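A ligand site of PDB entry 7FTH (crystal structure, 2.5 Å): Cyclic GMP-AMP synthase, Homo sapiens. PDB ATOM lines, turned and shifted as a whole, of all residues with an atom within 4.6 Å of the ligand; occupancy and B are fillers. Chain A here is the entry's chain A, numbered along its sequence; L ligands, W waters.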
ATOM      1  N   ASP A  67      10.176   1.848 -15.429  1.00  0.00           N
ATOM      2  CA  ASP A  67      10.240   3.113 -16.144  1.00  0.00           C
ATOM      3  C   ASP A  67       8.832   3.605 -16.481  1.00  0.00           C
ATOM      4  O   ASP A  67       8.100   2.931 -17.203  1.00  0.00           O
ATOM      5  CB  ASP A  67      11.096   2.944 -17.400  1.00  0.00           C
ATOM      6  CG  ASP A  67      10.880   4.035 -18.436  1.00  0.00           C
ATOM      7  OD1 ASP A  67      10.020   3.842 -19.321  1.00  0.00           O
ATOM      8  OD2 ASP A  67      11.559   5.087 -18.340  1.00  0.00           O
ATOM      9  N   TYR A  88      17.789  18.756 -28.750  1.00  0.00           N
ATOM     10  CA  TYR A  88      17.554  19.592 -27.576  1.00  0.00           C
ATOM     11  C   TYR A  88      16.901  20.909 -27.969  1.00  0.00           C
ATOM     12  O   TYR A  88      17.357  21.577 -28.911  1.00  0.00           O
ATOM     13  CB  TYR A  88      18.860  19.851 -26.830  1.00  0.00           C
ATOM     14  CG  TYR A  88      19.419  18.634 -26.146  1.00  0.00           C
ATOM     15  CD1 TYR A  88      20.378  17.842 -26.758  1.00  0.00           C
ATOM     16  CD2 TYR A  88      18.963  18.244 -24.889  1.00  0.00           C
ATOM     17  CE1 TYR A  88      20.892  16.708 -26.135  1.00  0.00           C
ATOM     18  CE2 TYR A  88      19.464  17.133 -24.252  1.00  0.00           C
ATOM     19  CZ  TYR A  88      20.434  16.367 -24.875  1.00  0.00           C
ATOM     20  OH  TYR A  88      20.916  15.251 -24.248  1.00  0.00           O
ATOM     21  N   ARG A 142      21.660  11.063 -10.689  1.00  0.00           N
ATOM     22  CA  ARG A 142      22.485  10.924 -11.876  1.00  0.00           C
ATOM     23  C   ARG A 142      22.532  12.217 -12.688  1.00  0.00           C
ATOM     24  O   ARG A 142      21.833  13.196 -12.414  1.00  0.00           O
ATOM     25  CB  ARG A 142      22.011   9.751 -12.724  1.00  0.00           C
ATOM     26  CG  ARG A 142      22.531   8.456 -12.191  1.00  0.00           C
ATOM     27  CD  ARG A 142      22.535   7.414 -13.274  1.00  0.00           C
ATOM     28  NE  ARG A 142      22.679   6.083 -12.691  1.00  0.00           N
ATOM     29  CZ  ARG A 142      22.271   4.965 -13.289  1.00  0.00           C
ATOM     30  NH1 ARG A 142      21.699   5.010 -14.489  1.00  0.00           N
ATOM     31  NH2 ARG A 142      22.448   3.794 -12.683  1.00  0.00           N
ATOM     32  N   GLY A 143      23.342  12.183 -13.746  1.00  0.00           N
ATOM     33  CA  GLY A 143      23.899  13.374 -14.348  1.00  0.00           C
ATOM     34  C   GLY A 143      22.952  14.134 -15.248  1.00  0.00           C
ATOM     35  O   GLY A 143      23.009  14.007 -16.473  1.00  0.00           O
ATOM     36  N   SER A 145      19.775  13.724 -15.572  1.00  0.00           N
ATOM     37  CA  SER A 145      18.692  12.886 -16.065  1.00  0.00           C
ATOM     38  C   SER A 145      17.346  13.577 -15.854  1.00  0.00           C
ATOM     39  O   SER A 145      17.169  14.324 -14.878  1.00  0.00           O
ATOM     40  CB  SER A 145      18.687  11.540 -15.337  1.00  0.00           C
ATOM     41  OG  SER A 145      17.539  10.763 -15.657  1.00  0.00           O
ATOM     42  N   PRO A 146      16.370  13.347 -16.737  1.00  0.00           N
ATOM     43  CA  PRO A 146      15.018  13.840 -16.507  1.00  0.00           C
ATOM     44  C   PRO A 146      14.219  12.981 -15.549  1.00  0.00           C
ATOM     45  O   PRO A 146      13.053  13.287 -15.282  1.00  0.00           O
ATOM     46  CB  PRO A 146      14.418  13.770 -17.915  1.00  0.00           C
ATOM     47  CG  PRO A 146      15.022  12.545 -18.468  1.00  0.00           C
ATOM     48  CD  PRO A 146      16.457  12.553 -17.976  1.00  0.00           C
ATOM     49  N   ALA A 147      14.827  11.923 -15.029  1.00  0.00           N
ATOM     50  CA  ALA A 147      14.139  10.887 -14.270  1.00  0.00           C
ATOM     51  C   ALA A 147      14.230  11.148 -12.768  1.00  0.00           C
ATOM     52  O   ALA A 147      15.328  11.223 -12.211  1.00  0.00           O
ATOM     53  CB  ALA A 147      14.721   9.514 -14.613  1.00  0.00           C
ATOM     54  N   ASP A 159      11.952   4.750 -12.528  1.00  0.00           N
ATOM     55  CA  ASP A 159      12.212   6.036 -13.175  1.00  0.00           C
ATOM     56  C   ASP A 159      10.879   6.663 -13.580  1.00  0.00           C
ATOM     57  O   ASP A 159      10.128   6.083 -14.362  1.00  0.00           O
ATOM     58  CB  ASP A 159      13.087   5.851 -14.432  1.00  0.00           C
ATOM     59  CG  ASP A 159      14.573   5.946 -14.133  1.00  0.00           C
ATOM     60  OD1 ASP A 159      14.952   5.889 -12.950  1.00  0.00           O
ATOM     61  OD2 ASP A 159      15.355   6.071 -15.098  1.00  0.00           O
ATOM     62  N   THR A 161       9.261  10.051 -15.383  1.00  0.00           N
ATOM     63  CA  THR A 161       9.651  11.150 -16.261  1.00  0.00           C
ATOM     64  C   THR A 161       8.446  12.008 -16.596  1.00  0.00           C
ATOM     65  O   THR A 161       7.413  11.499 -17.033  1.00  0.00           O
ATOM     66  CB  THR A 161      10.313  10.646 -17.538  1.00  0.00           C
ATOM     67  OG1 THR A 161      11.653  10.232 -17.237  1.00  0.00           O
ATOM     68  CG2 THR A 161      10.391  11.740 -18.523  1.00  0.00           C
ATOM     69  N   VAL A 200      11.105  15.916 -22.842  1.00  0.00           N
ATOM     70  CA  VAL A 200      11.389  15.536 -21.461  1.00  0.00           C
ATOM     71  C   VAL A 200      12.492  16.440 -20.912  1.00  0.00           C
ATOM     72  O   VAL A 200      13.356  16.920 -21.674  1.00  0.00           O
ATOM     73  CB  VAL A 200      11.757  14.053 -21.386  1.00  0.00           C
ATOM     74  CG1 VAL A 200      10.654  13.254 -22.016  1.00  0.00           C
ATOM     75  CG2 VAL A 200      13.025  13.797 -22.130  1.00  0.00           C
ATOM     76  N   LYS A 202      15.402  16.556 -19.788  1.00  0.00           N
ATOM     77  CA  LYS A 202      16.838  16.337 -19.768  1.00  0.00           C
ATOM     78  C   LYS A 202      17.525  17.556 -20.368  1.00  0.00           C
ATOM     79  O   LYS A 202      17.280  17.910 -21.515  1.00  0.00           O
ATOM     80  CB  LYS A 202      17.220  15.078 -20.531  1.00  0.00           C
ATOM     81  CG  LYS A 202      18.583  15.170 -21.193  1.00  0.00           C
ATOM     82  CD  LYS A 202      19.510  14.080 -20.726  1.00  0.00           C
ATOM     83  CE  LYS A 202      20.919  14.629 -20.648  1.00  0.00           C
ATOM     84  NZ  LYS A 202      20.908  15.896 -19.856  1.00  0.00           N
ATOM     85  N   ARG A 216      14.369  17.808 -24.274  1.00  0.00           N
ATOM     86  CA  ARG A 216      14.911  16.905 -25.275  1.00  0.00           C
ATOM     87  C   ARG A 216      13.790  16.010 -25.792  1.00  0.00           C
ATOM     88  O   ARG A 216      12.898  15.637 -25.036  1.00  0.00           O
ATOM     89  CB  ARG A 216      16.039  16.055 -24.713  1.00  0.00           C
ATOM     90  CG  ARG A 216      16.859  15.419 -25.780  1.00  0.00           C
ATOM     91  CD  ARG A 216      17.288  14.069 -25.318  1.00  0.00           C
ATOM     92  NE  ARG A 216      16.127  13.227 -25.083  1.00  0.00           N
ATOM     93  CZ  ARG A 216      16.095  12.259 -24.176  1.00  0.00           C
ATOM     94  NH1 ARG A 216      17.154  12.009 -23.410  1.00  0.00           N
ATOM     95  NH2 ARG A 216      14.998  11.532 -24.027  1.00  0.00           N
ATOM     96  N   LEU A 217      13.838  15.704 -27.091  1.00  0.00           N
ATOM     97  CA  LEU A 217      12.765  14.933 -27.700  1.00  0.00           C
ATOM     98  C   LEU A 217      12.791  13.491 -27.203  1.00  0.00           C
ATOM     99  O   LEU A 217      13.835  12.959 -26.797  1.00  0.00           O
ATOM    100  CB  LEU A 217      12.861  14.936 -29.218  1.00  0.00           C
ATOM    101  CG  LEU A 217      12.806  16.307 -29.911  1.00  0.00           C
ATOM    102  CD1 LEU A 217      13.283  16.145 -31.325  1.00  0.00           C
ATOM    103  CD2 LEU A 217      11.397  16.885 -29.900  1.00  0.00           C
ATOM    104  N   SER A 218      11.614  12.865 -27.215  1.00  0.00           N
ATOM    105  CA  SER A 218      11.416  11.474 -26.858  1.00  0.00           C
ATOM    106  C   SER A 218      10.308  10.887 -27.717  1.00  0.00           C
ATOM    107  O   SER A 218       9.385  11.587 -28.122  1.00  0.00           O
ATOM    108  CB  SER A 218      11.064  11.314 -25.367  1.00  0.00           C
ATOM    109  OG  SER A 218      10.588  10.016 -25.138  1.00  0.00           O
ATOM    110  N   SER A 220       9.257   7.320 -27.048  1.00  0.00           N
ATOM    111  CA  SER A 220       9.144   6.014 -26.450  1.00  0.00           C
ATOM    112  C   SER A 220       7.838   5.337 -26.791  1.00  0.00           C
ATOM    113  O   SER A 220       7.745   4.107 -26.757  1.00  0.00           O
ATOM    114  CB  SER A 220       9.314   6.153 -24.937  1.00  0.00           C
ATOM    115  OG  SER A 220      10.648   6.549 -24.663  1.00  0.00           O
ATOM    116  N   SER A 274      24.105   1.122 -22.100  1.00  0.00           N
ATOM    117  CA  SER A 274      22.712   1.232 -21.714  1.00  0.00           C
ATOM    118  C   SER A 274      21.862   0.421 -22.663  1.00  0.00           C
ATOM    119  O   SER A 274      22.184   0.289 -23.847  1.00  0.00           O
ATOM    120  CB  SER A 274      22.260   2.696 -21.727  1.00  0.00           C
ATOM    121  OG  SER A 274      20.931   2.849 -21.295  1.00  0.00           O
ATOM    122  N   TYR A 276      19.137   1.243 -23.918  1.00  0.00           N
ATOM    123  CA  TYR A 276      18.711   2.107 -25.017  1.00  0.00           C
ATOM    124  C   TYR A 276      19.668   2.017 -26.191  1.00  0.00           C
ATOM    125  O   TYR A 276      19.241   2.078 -27.339  1.00  0.00           O
ATOM    126  CB  TYR A 276      18.584   3.558 -24.565  1.00  0.00           C
ATOM    127  CG  TYR A 276      17.810   4.368 -25.561  1.00  0.00           C
ATOM    128  CD1 TYR A 276      16.422   4.225 -25.686  1.00  0.00           C
ATOM    129  CD2 TYR A 276      18.449   5.242 -26.412  1.00  0.00           C
ATOM    130  CE1 TYR A 276      15.725   4.933 -26.624  1.00  0.00           C
ATOM    131  CE2 TYR A 276      17.751   5.951 -27.350  1.00  0.00           C
ATOM    132  CZ  TYR A 276      16.399   5.798 -27.452  1.00  0.00           C
ATOM    133  OH  TYR A 276      15.755   6.539 -28.417  1.00  0.00           O
ATOM    134  N   HIS A 277      20.958   1.830 -25.918  1.00  0.00           N
ATOM    135  CA  HIS A 277      21.919   1.646 -27.005  1.00  0.00           C
ATOM    136  C   HIS A 277      21.656   0.340 -27.757  1.00  0.00           C
ATOM    137  O   HIS A 277      21.677   0.314 -28.988  1.00  0.00           O
ATOM    138  CB  HIS A 277      23.335   1.661 -26.459  1.00  0.00           C
ATOM    139  CG  HIS A 277      23.733   2.963 -25.851  1.00  0.00           C
ATOM    140  ND1 HIS A 277      24.196   3.058 -24.554  1.00  0.00           N
ATOM    141  CD2 HIS A 277      23.739   4.220 -26.339  1.00  0.00           C
ATOM    142  CE1 HIS A 277      24.482   4.327 -24.290  1.00  0.00           C
ATOM    143  NE2 HIS A 277      24.208   5.054 -25.354  1.00  0.00           N
ATOM    144  N   ASN A 322      20.722   7.905 -33.203  1.00  0.00           N
ATOM    145  CA  ASN A 322      19.384   7.871 -32.651  1.00  0.00           C
ATOM    146  C   ASN A 322      18.393   7.525 -33.770  1.00  0.00           C
ATOM    147  O   ASN A 322      18.470   8.080 -34.866  1.00  0.00           O
ATOM    148  CB  ASN A 322      19.051   9.212 -32.015  1.00  0.00           C
ATOM    149  CG  ASN A 322      17.634   9.317 -31.581  1.00  0.00           C
ATOM    150  OD1 ASN A 322      16.713   9.428 -32.402  1.00  0.00           O
ATOM    151  ND2 ASN A 322      17.432   9.271 -30.285  1.00  0.00           N
ATOM    152  N   PHE A 328      21.869  12.816 -34.341  1.00  0.00           N
ATOM    153  CA  PHE A 328      22.205  12.674 -32.943  1.00  0.00           C
ATOM    154  C   PHE A 328      22.954  11.355 -32.790  1.00  0.00           C
ATOM    155  O   PHE A 328      22.371  10.280 -32.973  1.00  0.00           O
ATOM    156  CB  PHE A 328      20.978  12.722 -32.044  1.00  0.00           C
ATOM    157  CG  PHE A 328      21.317  13.013 -30.628  1.00  0.00           C
ATOM    158  CD1 PHE A 328      21.427  14.315 -30.175  1.00  0.00           C
ATOM    159  CD2 PHE A 328      21.606  11.982 -29.746  1.00  0.00           C
ATOM    160  CE1 PHE A 328      21.773  14.587 -28.863  1.00  0.00           C
ATOM    161  CE2 PHE A 328      21.957  12.241 -28.431  1.00  0.00           C
ATOM    162  CZ  PHE A 328      22.043  13.547 -27.982  1.00  0.00           C
ATOM    163  N   LEU A 330      24.503   8.890 -30.477  1.00  0.00           N
ATOM    164  CA  LEU A 330      24.572   8.403 -29.104  1.00  0.00           C
ATOM    165  C   LEU A 330      25.980   7.972 -28.721  1.00  0.00           C
ATOM    166  O   LEU A 330      26.321   8.017 -27.546  1.00  0.00           O
ATOM    167  CB  LEU A 330      23.596   7.231 -28.934  1.00  0.00           C
ATOM    168  CG  LEU A 330      22.139   7.526 -29.290  1.00  0.00           C
ATOM    169  CD1 LEU A 330      21.311   6.258 -29.292  1.00  0.00           C
ATOM    170  CD2 LEU A 330      21.549   8.532 -28.304  1.00  0.00           C
ATOM    171  N   LEU A 335      29.712  12.212 -25.328  1.00  0.00           N
ATOM    172  CA  LEU A 335      28.898  11.395 -24.426  1.00  0.00           C
ATOM    173  C   LEU A 335      29.646  10.215 -23.825  1.00  0.00           C
ATOM    174  O   LEU A 335      29.427   9.876 -22.654  1.00  0.00           O
ATOM    175  CB  LEU A 335      27.686  10.844 -25.166  1.00  0.00           C
ATOM    176  CG  LEU A 335      26.661  11.844 -25.675  1.00  0.00           C
ATOM    177  CD1 LEU A 335      25.642  11.115 -26.525  1.00  0.00           C
ATOM    178  CD2 LEU A 335      25.985  12.534 -24.513  1.00  0.00           C
HETATM  179  C1  LIG L   1      16.014   9.199 -26.076  1.00  0.00           C
HETATM  180  N1  LIG L   1      13.629   7.650 -23.773  1.00  0.00           N
HETATM  181  C2  LIG L   1      14.946   8.014 -24.370  1.00  0.00           C
HETATM  182  N2  LIG L   1      14.879   8.802 -25.462  1.00  0.00           N
HETATM  183  N3  LIG L   1      17.224   8.796 -25.595  1.00  0.00           N
HETATM  184  C3  LIG L   1      17.303   8.010 -24.516  1.00  0.00           C
HETATM  185  C4  LIG L   1      16.170   7.603 -23.885  1.00  0.00           C
HETATM  186  N4  LIG L   1      16.548   6.823 -22.834  1.00  0.00           N
HETATM  187  C5  LIG L   1      17.907   6.739 -22.806  1.00  0.00           C
HETATM  188  N5  LIG L   1      18.350   7.471 -23.838  1.00  0.00           N
HETATM  189  C6  LIG L   1      19.732   7.723 -24.288  1.00  0.00           C
HETATM  190  C7  LIG L   1      20.295   9.012 -23.728  1.00  0.00           C
HETATM  191  O1  LIG L   1      20.735   9.894 -24.792  1.00  0.00           O
HETATM  192  C8  LIG L   1      21.395   8.620 -22.770  1.00  0.00           C
HETATM  193  C9  LIG L   1      21.769   7.322 -23.196  1.00  0.00           C
HETATM  194  C10 LIG L   1      22.107   6.480 -21.963  1.00  0.00           C
HETATM  195  O2  LIG L   1      21.372   7.051 -20.867  1.00  0.00           O
HETATM  196  P1  LIG L   1      20.897   6.056 -19.535  1.00  0.00           P
HETATM  197  O3  LIG L   1      20.189   4.829 -19.907  1.00  0.00           O
HETATM  198  O4  LIG L   1      20.145   6.986 -18.284  1.00  0.00           O
HETATM  199  C11 LIG L   1      20.515   8.357 -18.592  1.00  0.00           C
HETATM  200  C12 LIG L   1      21.711   8.782 -17.872  1.00  0.00           C
HETATM  201  O5  LIG L   1      21.588   8.355 -16.547  1.00  0.00           O
HETATM  202  C13 LIG L   1      21.642  10.299 -17.857  1.00  0.00           C
HETATM  203  C14 LIG L   1      22.240  10.960 -19.014  1.00  0.00           C
HETATM  204  O6  LIG L   1      22.519  10.022 -20.136  1.00  0.00           O
HETATM  205  P2  LIG L   1      22.456  10.844 -21.638  1.00  0.00           P
HETATM  206  O7  LIG L   1      22.540   9.550 -22.770  1.00  0.00           O
HETATM  207  O8  LIG L   1      21.133  11.541 -21.740  1.00  0.00           O
HETATM  208  O9  LIG L   1      23.467  11.943 -21.808  1.00  0.00           O
HETATM  209  O10 LIG L   1      20.182  10.559 -17.816  1.00  0.00           O
HETATM  210  C15 LIG L   1      19.553   9.235 -18.036  1.00  0.00           C
HETATM  211  N6  LIG L   1      18.393   9.344 -18.907  1.00  0.00           N
HETATM  212  C16 LIG L   1      18.695  10.138 -19.948  1.00  0.00           C
HETATM  213  N7  LIG L   1      17.577  10.210 -20.709  1.00  0.00           N
HETATM  214  C17 LIG L   1      17.131   8.931 -18.995  1.00  0.00           C
HETATM  215  C18 LIG L   1      16.617   9.472 -20.129  1.00  0.00           C
HETATM  216  C19 LIG L   1      15.198   9.181 -20.514  1.00  0.00           C
HETATM  217  N8  LIG L   1      14.391   8.335 -19.663  1.00  0.00           N
HETATM  218  C20 LIG L   1      14.940   7.778 -18.475  1.00  0.00           C
HETATM  219  N9  LIG L   1      14.122   6.906 -17.614  1.00  0.00           N
HETATM  220  N10 LIG L   1      16.313   8.052 -18.103  1.00  0.00           N
HETATM  221  O11 LIG L   1      14.725   9.664 -21.525  1.00  0.00           O
HETATM  222  O12 LIG L   1      22.141   5.607 -18.935  1.00  0.00           O
HETATM  223  O13 LIG L   1      20.621   6.673 -23.873  1.00  0.00           O
HETATM  224  O   HOH W   1      11.195   7.522 -17.026  1.00  0.00           O
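Arg 142 touches the ligand (CD to O5, 3.5 Å).
Pro 146 touches the ligand (CD to C18, 3.8 Å).
Lys 202 touches the ligand.
Tyr 276 touches the ligand (CE2 to N3, 3.4 Å).
His 277 touches the ligand.
CD2 of Leu 330 touches O1 of the ligand, 3.9 Å away.
Leu 335 touches the ligand (CD2 to O9, 3.7 Å).
Hydrophobic or aromatic side chains within 4 Å of the ligand: Pro 146, Tyr 276, His 277, Leu 330 and Leu 335.
The nearest printed residue that does not touch the ligand is Ala 147 (4.02 Å).
O3 of the ligand sits at hydrogen-bond distance from OG of Ser 274, 2.5 Å away.
The side-chain carboxylate (OD2) of Asp 159 lies within hydrogen-bond range of a nitrogen (N9) of the ligand (2.9 Å).
The side-chain hydroxyl (OG) of Ser 145 sits close to an oxygen (O10) of the ligand.
The guanidinium group (NH2) of Arg 216 sits at hydrogen-bond distance from a nitrogen (N2) of the ligand, 3.1 Å away.
N9 of the ligand lies within hydrogen-bond range of OD2 of Asp 67.
OG of Ser 220 is in hydrogen-bond range of N1 of the ligand.
A ring nitrogen (ND1) of His 277 sits at hydrogen-bond distance from the backbone NH (N) of Ser 274 (3.1 Å).
N of Ala 147 lies within hydrogen-bond range of OG of Ser 145 (3.0 Å).
N of Val 200 sits at hydrogen-bond distance from O of Arg 216, 2.8 Å away.
The side-chain hydroxyl (OG) of Ser 220 is in hydrogen-bond range of the side-chain hydroxyl (OG) of Ser 218.
Water W1 lies within hydrogen-bond range of the side-chain hydroxyl of Thr 161 (2.8 Å), the side-chain carboxylate of Asp 67 (2.8 Å), a nitrogen (N9) of the ligand (3.0 Å) and the backbone carbonyl oxygen of Asp 159 (3.2 Å).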
